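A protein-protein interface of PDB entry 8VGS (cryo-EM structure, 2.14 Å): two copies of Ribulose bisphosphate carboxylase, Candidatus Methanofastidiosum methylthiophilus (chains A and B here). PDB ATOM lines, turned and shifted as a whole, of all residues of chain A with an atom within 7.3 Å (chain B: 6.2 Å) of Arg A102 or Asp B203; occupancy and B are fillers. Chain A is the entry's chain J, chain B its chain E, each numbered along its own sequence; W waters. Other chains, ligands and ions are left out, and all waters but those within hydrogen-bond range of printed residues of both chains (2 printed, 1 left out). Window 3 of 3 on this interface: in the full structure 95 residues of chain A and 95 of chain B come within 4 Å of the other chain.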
ATOM      1  N   PHE A  73     -39.410  19.341  -7.447  1.00  0.00           N
ATOM      2  CA  PHE A  73     -38.937  19.924  -8.698  1.00  0.00           C
ATOM      3  C   PHE A  73     -37.595  19.338  -9.114  1.00  0.00           C
ATOM      4  O   PHE A  73     -37.338  19.168 -10.310  1.00  0.00           O
ATOM      5  CB  PHE A  73     -38.834  21.444  -8.567  1.00  0.00           C
ATOM      6  CG  PHE A  73     -38.526  22.147  -9.860  1.00  0.00           C
ATOM      7  CD1 PHE A  73     -39.539  22.457 -10.753  1.00  0.00           C
ATOM      8  CD2 PHE A  73     -37.226  22.506 -10.179  1.00  0.00           C
ATOM      9  CE1 PHE A  73     -39.262  23.106 -11.940  1.00  0.00           C
ATOM     10  CE2 PHE A  73     -36.943  23.154 -11.366  1.00  0.00           C
ATOM     11  CZ  PHE A  73     -37.961  23.455 -12.247  1.00  0.00           C
ATOM     12  N   MET A  77     -36.007  16.826 -12.815  1.00  0.00           N
ATOM     13  CA  MET A  77     -34.778  16.934 -13.588  1.00  0.00           C
ATOM     14  C   MET A  77     -33.931  15.671 -13.529  1.00  0.00           C
ATOM     15  O   MET A  77     -32.820  15.666 -14.069  1.00  0.00           O
ATOM     16  CB  MET A  77     -33.955  18.131 -13.100  1.00  0.00           C
ATOM     17  CG  MET A  77     -34.733  19.438 -13.043  1.00  0.00           C
ATOM     18  SD  MET A  77     -34.961  20.197 -14.661  1.00  0.00           S
ATOM     19  CE  MET A  77     -36.385  19.296 -15.269  1.00  0.00           C
ATOM     20  N   TRP A  97     -33.155  18.246 -20.935  1.00  0.00           N
ATOM     21  CA  TRP A  97     -32.184  19.251 -21.357  1.00  0.00           C
ATOM     22  C   TRP A  97     -32.391  20.591 -20.662  1.00  0.00           C
ATOM     23  O   TRP A  97     -31.591  21.510 -20.871  1.00  0.00           O
ATOM     24  CB  TRP A  97     -32.199  19.409 -22.883  1.00  0.00           C
ATOM     25  CG  TRP A  97     -33.500  19.822 -23.500  1.00  0.00           C
ATOM     26  CD1 TRP A  97     -34.423  19.005 -24.084  1.00  0.00           C
ATOM     27  CD2 TRP A  97     -33.989  21.159 -23.663  1.00  0.00           C
ATOM     28  NE1 TRP A  97     -35.474  19.745 -24.568  1.00  0.00           N
ATOM     29  CE2 TRP A  97     -35.230  21.071 -24.325  1.00  0.00           C
ATOM     30  CE3 TRP A  97     -33.507  22.420 -23.301  1.00  0.00           C
ATOM     31  CZ2 TRP A  97     -35.995  22.194 -24.631  1.00  0.00           C
ATOM     32  CZ3 TRP A  97     -34.268  23.535 -23.605  1.00  0.00           C
ATOM     33  CH2 TRP A  97     -35.497  23.414 -24.264  1.00  0.00           C
ATOM     34  N   ARG A  98     -33.434  20.712 -19.835  1.00  0.00           N
ATOM     35  CA  ARG A  98     -33.521  21.792 -18.859  1.00  0.00           C
ATOM     36  C   ARG A  98     -32.320  21.819 -17.918  1.00  0.00           C
ATOM     37  O   ARG A  98     -31.956  22.887 -17.411  1.00  0.00           O
ATOM     38  CB  ARG A  98     -34.808  21.643 -18.047  1.00  0.00           C
ATOM     39  CG  ARG A  98     -35.432  22.949 -17.633  1.00  0.00           C
ATOM     40  CD  ARG A  98     -36.946  22.889 -17.659  1.00  0.00           C
ATOM     41  NE  ARG A  98     -37.525  24.006 -16.925  1.00  0.00           N
ATOM     42  CZ  ARG A  98     -38.552  23.905 -16.094  1.00  0.00           C
ATOM     43  NH1 ARG A  98     -39.159  22.748 -15.883  1.00  0.00           N
ATOM     44  NH2 ARG A  98     -38.980  24.990 -15.457  1.00  0.00           N
ATOM     45  N   LEU A  99     -31.712  20.656 -17.652  1.00  0.00           N
ATOM     46  CA  LEU A  99     -30.508  20.588 -16.827  1.00  0.00           C
ATOM     47  C   LEU A  99     -29.377  21.435 -17.395  1.00  0.00           C
ATOM     48  O   LEU A  99     -28.578  21.993 -16.635  1.00  0.00           O
ATOM     49  CB  LEU A  99     -30.039  19.138 -16.703  1.00  0.00           C
ATOM     50  CG  LEU A  99     -30.877  18.134 -15.910  1.00  0.00           C
ATOM     51  CD1 LEU A  99     -30.555  16.719 -16.361  1.00  0.00           C
ATOM     52  CD2 LEU A  99     -30.635  18.290 -14.421  1.00  0.00           C
ATOM     53  N   PHE A 100     -29.303  21.556 -18.716  1.00  0.00           N
ATOM     54  CA  PHE A 100     -28.150  22.153 -19.369  1.00  0.00           C
ATOM     55  C   PHE A 100     -28.182  23.673 -19.260  1.00  0.00           C
ATOM     56  O   PHE A 100     -29.246  24.294 -19.211  1.00  0.00           O
ATOM     57  CB  PHE A 100     -28.101  21.727 -20.837  1.00  0.00           C
ATOM     58  CG  PHE A 100     -28.120  20.237 -21.030  1.00  0.00           C
ATOM     59  CD1 PHE A 100     -27.407  19.406 -20.180  1.00  0.00           C
ATOM     60  CD2 PHE A 100     -28.858  19.663 -22.052  1.00  0.00           C
ATOM     61  CE1 PHE A 100     -27.422  18.035 -20.350  1.00  0.00           C
ATOM     62  CE2 PHE A 100     -28.877  18.292 -22.227  1.00  0.00           C
ATOM     63  CZ  PHE A 100     -28.158  17.477 -21.375  1.00  0.00           C
ATOM     64  N   ASP A 101     -26.988  24.263 -19.200  1.00  0.00           N
ATOM     65  CA  ASP A 101     -26.851  25.713 -19.120  1.00  0.00           C
ATOM     66  C   ASP A 101     -27.456  26.378 -20.348  1.00  0.00           C
ATOM     67  O   ASP A 101     -27.238  25.941 -21.481  1.00  0.00           O
ATOM     68  CB  ASP A 101     -25.376  26.094 -18.984  1.00  0.00           C
ATOM     69  CG  ASP A 101     -25.164  27.597 -18.904  1.00  0.00           C
ATOM     70  OD1 ASP A 101     -25.940  28.274 -18.199  1.00  0.00           O
ATOM     71  OD2 ASP A 101     -24.216  28.099 -19.542  1.00  0.00           O
ATOM     72  N   ARG A 102     -28.215  27.445 -20.118  1.00  0.00           N
ATOM     73  CA  ARG A 102     -28.878  28.138 -21.208  1.00  0.00           C
ATOM     74  C   ARG A 102     -27.859  28.916 -22.039  1.00  0.00           C
ATOM     75  O   ARG A 102     -26.714  29.135 -21.633  1.00  0.00           O
ATOM     76  CB  ARG A 102     -29.961  29.070 -20.667  1.00  0.00           C
ATOM     77  CG  ARG A 102     -31.189  28.339 -20.151  1.00  0.00           C
ATOM     78  CD  ARG A 102     -31.573  27.185 -21.062  1.00  0.00           C
ATOM     79  NE  ARG A 102     -32.704  26.432 -20.533  1.00  0.00           N
ATOM     80  CZ  ARG A 102     -33.851  26.250 -21.171  1.00  0.00           C
ATOM     81  NH1 ARG A 102     -34.056  26.745 -22.380  1.00  0.00           N
ATOM     82  NH2 ARG A 102     -34.817  25.552 -20.580  1.00  0.00           N
ATOM     83  N   GLY A 103     -28.292  29.337 -23.225  1.00  0.00           N
ATOM     84  CA  GLY A 103     -27.408  30.033 -24.134  1.00  0.00           C
ATOM     85  C   GLY A 103     -26.536  29.144 -24.989  1.00  0.00           C
ATOM     86  O   GLY A 103     -25.474  29.585 -25.438  1.00  0.00           O
ATOM     87  N   GLY A 104     -26.952  27.903 -25.235  1.00  0.00           N
ATOM     88  CA  GLY A 104     -26.192  27.001 -26.079  1.00  0.00           C
ATOM     89  C   GLY A 104     -24.835  26.603 -25.533  1.00  0.00           C
ATOM     90  O   GLY A 104     -23.836  26.642 -26.257  1.00  0.00           O
ATOM     91  N   ASN A 105     -24.785  26.221 -24.259  1.00  0.00           N
ATOM     92  CA  ASN A 105     -23.546  25.813 -23.603  1.00  0.00           C
ATOM     93  C   ASN A 105     -23.331  24.320 -23.848  1.00  0.00           C
ATOM     94  O   ASN A 105     -24.033  23.482 -23.273  1.00  0.00           O
ATOM     95  CB  ASN A 105     -23.614  26.137 -22.112  1.00  0.00           C
ATOM     96  CG  ASN A 105     -22.274  25.995 -21.406  1.00  0.00           C
ATOM     97  OD1 ASN A 105     -21.352  25.356 -21.906  1.00  0.00           O
ATOM     98  ND2 ASN A 105     -22.168  26.597 -20.228  1.00  0.00           N
ATOM     99  N   ASN A 108     -21.259  22.480 -20.893  1.00  0.00           N
ATOM    100  CA  ASN A 108     -22.146  22.101 -19.798  1.00  0.00           C
ATOM    101  C   ASN A 108     -22.768  20.727 -20.032  1.00  0.00           C
ATOM    102  O   ASN A 108     -22.853  19.909 -19.105  1.00  0.00           O
ATOM    103  CB  ASN A 108     -23.222  23.173 -19.623  1.00  0.00           C
ATOM    104  CG  ASN A 108     -24.154  22.884 -18.475  1.00  0.00           C
ATOM    105  OD1 ASN A 108     -25.174  22.221 -18.647  1.00  0.00           O
ATOM    106  ND2 ASN A 108     -23.809  23.372 -17.290  1.00  0.00           N
ATOM    107  N   ALA A 136     -36.493  20.547 -30.196  1.00  0.00           N
ATOM    108  CA  ALA A 136     -36.645  21.621 -29.218  1.00  0.00           C
ATOM    109  C   ALA A 136     -35.315  21.946 -28.550  1.00  0.00           C
ATOM    110  O   ALA A 136     -35.016  23.115 -28.282  1.00  0.00           O
ATOM    111  CB  ALA A 136     -37.692  21.236 -28.174  1.00  0.00           C
ATOM    112  N   GLN A 140     -31.950  25.402 -29.243  1.00  0.00           N
ATOM    113  CA  GLN A 140     -31.189  26.142 -28.244  1.00  0.00           C
ATOM    114  C   GLN A 140     -29.735  26.381 -28.634  1.00  0.00           C
ATOM    115  O   GLN A 140     -29.059  27.166 -27.962  1.00  0.00           O
ATOM    116  CB  GLN A 140     -31.227  25.404 -26.903  1.00  0.00           C
ATOM    117  CG  GLN A 140     -32.618  25.202 -26.332  1.00  0.00           C
ATOM    118  CD  GLN A 140     -33.176  26.463 -25.705  1.00  0.00           C
ATOM    119  OE1 GLN A 140     -32.523  27.097 -24.875  1.00  0.00           O
ATOM    120  NE2 GLN A 140     -34.388  26.833 -26.097  1.00  0.00           N
ATOM    121  N   TYR A 141     -29.235  25.742 -29.687  1.00  0.00           N
ATOM    122  CA  TYR A 141     -27.809  25.742 -29.976  1.00  0.00           C
ATOM    123  C   TYR A 141     -27.547  26.308 -31.364  1.00  0.00           C
ATOM    124  O   TYR A 141     -28.393  26.225 -32.260  1.00  0.00           O
ATOM    125  CB  TYR A 141     -27.229  24.325 -29.840  1.00  0.00           C
ATOM    126  CG  TYR A 141     -27.329  23.806 -28.422  1.00  0.00           C
ATOM    127  CD1 TYR A 141     -28.478  23.167 -27.979  1.00  0.00           C
ATOM    128  CD2 TYR A 141     -26.286  23.975 -27.520  1.00  0.00           C
ATOM    129  CE1 TYR A 141     -28.591  22.707 -26.688  1.00  0.00           C
ATOM    130  CE2 TYR A 141     -26.389  23.515 -26.218  1.00  0.00           C
ATOM    131  CZ  TYR A 141     -27.547  22.882 -25.810  1.00  0.00           C
ATOM    132  OH  TYR A 141     -27.669  22.416 -24.523  1.00  0.00           O
ATOM    133  N   ARG A 279     -19.252  32.034 -32.553  1.00  0.00           N
ATOM    134  CA  ARG A 279     -20.136  33.182 -32.373  1.00  0.00           C
ATOM    135  C   ARG A 279     -19.475  34.492 -32.792  1.00  0.00           C
ATOM    136  O   ARG A 279     -20.129  35.350 -33.395  1.00  0.00           O
ATOM    137  CB  ARG A 279     -20.609  33.252 -30.922  1.00  0.00           C
ATOM    138  CG  ARG A 279     -21.441  32.049 -30.508  1.00  0.00           C
ATOM    139  CD  ARG A 279     -21.655  31.989 -29.007  1.00  0.00           C
ATOM    140  NE  ARG A 279     -22.449  30.824 -28.632  1.00  0.00           N
ATOM    141  CZ  ARG A 279     -23.111  30.701 -27.491  1.00  0.00           C
ATOM    142  NH1 ARG A 279     -23.088  31.652 -26.572  1.00  0.00           N
ATOM    143  NH2 ARG A 279     -23.815  29.595 -27.266  1.00  0.00           N
ATOM    144  N   ALA B 200     -25.074  26.293 -13.504  1.00  0.00           N
ATOM    145  CA  ALA B 200     -24.866  27.417 -14.405  1.00  0.00           C
ATOM    146  C   ALA B 200     -26.170  28.203 -14.476  1.00  0.00           C
ATOM    147  O   ALA B 200     -27.022  28.094 -13.588  1.00  0.00           O
ATOM    148  CB  ALA B 200     -24.372  26.918 -15.774  1.00  0.00           C
ATOM    149  N   ASN B 201     -26.322  29.020 -15.520  1.00  0.00           N
ATOM    150  CA  ASN B 201     -27.533  29.818 -15.719  1.00  0.00           C
ATOM    151  C   ASN B 201     -28.644  28.955 -16.326  1.00  0.00           C
ATOM    152  O   ASN B 201     -29.084  29.141 -17.462  1.00  0.00           O
ATOM    153  CB  ASN B 201     -27.229  31.028 -16.592  1.00  0.00           C
ATOM    154  CG  ASN B 201     -28.407  31.975 -16.707  1.00  0.00           C
ATOM    155  OD1 ASN B 201     -29.076  32.277 -15.719  1.00  0.00           O
ATOM    156  ND2 ASN B 201     -28.669  32.446 -17.919  1.00  0.00           N
ATOM    157  N   GLN B 202     -29.094  27.981 -15.540  1.00  0.00           N
ATOM    158  CA  GLN B 202     -30.290  27.237 -15.895  1.00  0.00           C
ATOM    159  C   GLN B 202     -31.524  28.113 -15.694  1.00  0.00           C
ATOM    160  O   GLN B 202     -31.523  29.060 -14.906  1.00  0.00           O
ATOM    161  CB  GLN B 202     -30.404  25.951 -15.071  1.00  0.00           C
ATOM    162  CG  GLN B 202     -29.580  24.782 -15.608  1.00  0.00           C
ATOM    163  CD  GLN B 202     -28.136  24.802 -15.137  1.00  0.00           C
ATOM    164  OE1 GLN B 202     -27.769  25.581 -14.261  1.00  0.00           O
ATOM    165  NE2 GLN B 202     -27.312  23.941 -15.721  1.00  0.00           N
ATOM    166  N   ASP B 203     -32.587  27.786 -16.433  1.00  0.00           N
ATOM    167  CA  ASP B 203     -33.772  28.639 -16.439  1.00  0.00           C
ATOM    168  C   ASP B 203     -34.487  28.650 -15.091  1.00  0.00           C
ATOM    169  O   ASP B 203     -35.110  29.657 -14.737  1.00  0.00           O
ATOM    170  CB  ASP B 203     -34.719  28.207 -17.561  1.00  0.00           C
ATOM    171  CG  ASP B 203     -35.619  27.061 -17.158  1.00  0.00           C
ATOM    172  OD1 ASP B 203     -36.718  27.314 -16.623  1.00  0.00           O
ATOM    173  OD2 ASP B 203     -35.219  25.903 -17.372  1.00  0.00           O
ATOM    174  N   PHE B 204     -34.412  27.562 -14.325  1.00  0.00           N
ATOM    175  CA  PHE B 204     -35.067  27.524 -13.024  1.00  0.00           C
ATOM    176  C   PHE B 204     -34.184  28.056 -11.906  1.00  0.00           C
ATOM    177  O   PHE B 204     -34.700  28.406 -10.839  1.00  0.00           O
ATOM    178  CB  PHE B 204     -35.518  26.097 -12.689  1.00  0.00           C
ATOM    179  CG  PHE B 204     -34.475  25.048 -12.948  1.00  0.00           C
ATOM    180  CD1 PHE B 204     -33.512  24.761 -11.995  1.00  0.00           C
ATOM    181  CD2 PHE B 204     -34.461  24.343 -14.140  1.00  0.00           C
ATOM    182  CE1 PHE B 204     -32.555  23.796 -12.226  1.00  0.00           C
ATOM    183  CE2 PHE B 204     -33.503  23.378 -14.377  1.00  0.00           C
ATOM    184  CZ  PHE B 204     -32.549  23.103 -13.419  1.00  0.00           C
ATOM    185  N   CYS B 205     -32.874  28.122 -12.126  1.00  0.00           N
ATOM    186  CA  CYS B 205     -31.927  28.708 -11.180  1.00  0.00           C
ATOM    187  C   CYS B 205     -31.074  29.721 -11.931  1.00  0.00           C
ATOM    188  O   CYS B 205     -29.937  29.430 -12.319  1.00  0.00           O
ATOM    189  CB  CYS B 205     -31.068  27.631 -10.516  1.00  0.00           C
ATOM    190  SG  CYS B 205     -30.332  26.429 -11.655  1.00  0.00           S
ATOM    191  N   PRO B 206     -31.618  30.914 -12.188  1.00  0.00           N
ATOM    192  CA  PRO B 206     -30.868  31.931 -12.938  1.00  0.00           C
ATOM    193  C   PRO B 206     -29.595  32.339 -12.213  1.00  0.00           C
ATOM    194  O   PRO B 206     -29.561  32.435 -10.985  1.00  0.00           O
ATOM    195  CB  PRO B 206     -31.857  33.099 -13.044  1.00  0.00           C
ATOM    196  CG  PRO B 206     -33.200  32.504 -12.755  1.00  0.00           C
ATOM    197  CD  PRO B 206     -32.955  31.389 -11.795  1.00  0.00           C
ATOM    198  N   ALA B 238     -20.874  29.035 -22.165  1.00  0.00           N
ATOM    199  CA  ALA B 238     -20.801  28.642 -23.567  1.00  0.00           C
ATOM    200  C   ALA B 238     -19.572  29.239 -24.241  1.00  0.00           C
ATOM    201  O   ALA B 238     -18.899  28.568 -25.031  1.00  0.00           O
ATOM    202  CB  ALA B 238     -22.076  29.061 -24.298  1.00  0.00           C
ATOM    203  N   THR B 242     -19.760  35.038 -21.890  1.00  0.00           N
ATOM    204  CA  THR B 242     -20.643  34.622 -20.809  1.00  0.00           C
ATOM    205  C   THR B 242     -19.861  34.338 -19.531  1.00  0.00           C
ATOM    206  O   THR B 242     -20.317  34.679 -18.434  1.00  0.00           O
ATOM    207  CB  THR B 242     -21.447  33.395 -21.235  1.00  0.00           C
ATOM    208  OG1 THR B 242     -22.073  33.650 -22.498  1.00  0.00           O
ATOM    209  CG2 THR B 242     -22.515  33.077 -20.203  1.00  0.00           C
ATOM    210  N   ARG B 246     -20.390  36.372 -16.071  1.00  0.00           N
ATOM    211  CA  ARG B 246     -20.707  35.743 -14.794  1.00  0.00           C
ATOM    212  C   ARG B 246     -19.669  36.091 -13.731  1.00  0.00           C
ATOM    213  O   ARG B 246     -20.013  36.316 -12.563  1.00  0.00           O
ATOM    214  CB  ARG B 246     -20.820  34.231 -14.987  1.00  0.00           C
ATOM    215  CG  ARG B 246     -21.884  33.859 -16.009  1.00  0.00           C
ATOM    216  CD  ARG B 246     -22.172  32.372 -16.072  1.00  0.00           C
ATOM    217  NE  ARG B 246     -23.330  32.111 -16.919  1.00  0.00           N
ATOM    218  CZ  ARG B 246     -23.523  30.996 -17.610  1.00  0.00           C
ATOM    219  NH1 ARG B 246     -22.664  29.993 -17.559  1.00  0.00           N
ATOM    220  NH2 ARG B 246     -24.603  30.890 -18.379  1.00  0.00           N
HETATM  221  O   HOH W   1     -24.067  32.196 -23.875  1.00  0.00           O
HETATM  222  O   HOH W   2     -32.514  25.212 -17.777  1.00  0.00           O
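The backbone NH of Asn B201 lies within hydrogen-bond range of the side-chain carboxylate of Asp A101.
The backbone carbonyl oxygen (O) of Asn B201 lies within hydrogen-bond range of the backbone NH (N) of Arg A102, at 3.3 Å.
NE2 of Gln B202 lies within hydrogen-bond range of O of Leu A99 (2.5 Å).
The guanidinium group (NE) of Arg A98 lies within salt-bridge range of the side-chain carboxylate (OD2) of Asp B203.
The side-chain carboxylate (OD2) of Asp B203 lies within salt-bridge range of the guanidinium group (NH2) of Arg A102, 3.3 Å away.
N of Ala B238 sits close to ND2 of Asn A105 (3.4 Å).
OD1 of Asp A101 lies within salt-bridge range of NH2 of Arg B246 (2.9 Å).
The side-chain amide oxygen of Gln B202 sits close to the backbone carbonyl oxygen of Ala B200.
OE1 of Gln B202 lies close to SG of Cys B205 (3.8 Å).
The side-chain amide nitrogen of Asn A105 is in hydrogen-bond range of the side-chain carboxylate of Asp A101 (2.6 Å).
The backbone NH (N) of Asp A101 lies within hydrogen-bond range of the side-chain amide oxygen (OD1) of Asn A108 (2.8 Å).
The side-chain amide oxygen of Gln A140 sits at hydrogen-bond distance from the guanidinium group of Arg A102.
The guanidinium group (NH2) of Arg A279 sits at hydrogen-bond distance from the backbone carbonyl oxygen (O) of Gly A104, 3.1 Å away.
Among the printed residues, merely in contact across the chains: Asp A101 with Ala B200, Arg A98 with Phe B204, Arg A279 with Ala B238, Phe A73 with Phe B204, Asp A101 with Gln B202, Met A77 with Phe B204, Arg A98 with Gln B202, Gly A104 with Ala B238, Gly A103 with Ala B238, Phe A100 with Gln B202, Asn A108 with Gln B202 and Asn A108 with Ala B200.
Arg A102 touches two residues of chain B.
Printed residues of chain B within 4 Å of Gly A104: Ala B238.
Printed residues of chain A within 4 Å of Asn B201: Asp A101 (2.8 Å) and Arg A102 (3.3 Å).
Pro B206 touches none of the printed residues of chain A.
Of the printed residues of chain A, Arg B246 touches Asp A101.
The nearest residue of chain B that does not touch Arg A102 is Arg B246 (4.3 Å).
The nearest residue of chain A that does not touch Asp B203 is Phe A100 (5.6 Å).
The nearest printed residue of chain B that does not touch Arg A279 is Thr B242 (4.6 Å).
Hydrophobic or aromatic side chains of chain A within 4 Å of the printed part of chain B: Phe A73 and Met A77.
Printed residues of chain B that touch a printed residue of chain A: Ala B200, Asn B201, Gln B202, Asp B203, Phe B204, Ala B238 and Arg B246.
Hydrophobic or aromatic side chains of chain B within 4 Å of the printed part of chain A: Ala B200, Phe B204 and Ala B238.
Among the printed residues, 19 pairs touch across the chains.
Among the printed residues, Asp or Glu carboxylates within 4 Å of a Lys or Arg side-chain nitrogen of the other chain: Arg A98 with Asp B203, Asp A101 with Arg B246 and Arg A102 with Asp B203.
No position is printed for both chains.
Of the 19 pairs that touch across the chains among the printed residues, none has its exchanged pair printed and touching as well.
Water W2 lies within hydrogen-bond range of O of Arg A98 (2.4 Å), OD2 of Asp B203 (2.8 Å) and NE of Arg A102 (3.0 Å).
Water W1 lies within hydrogen-bond range of OG1 of Thr B242 (2.8 Å), NH1 of Arg A279 (2.9 Å) and O of Gly A103 (3.4 Å).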
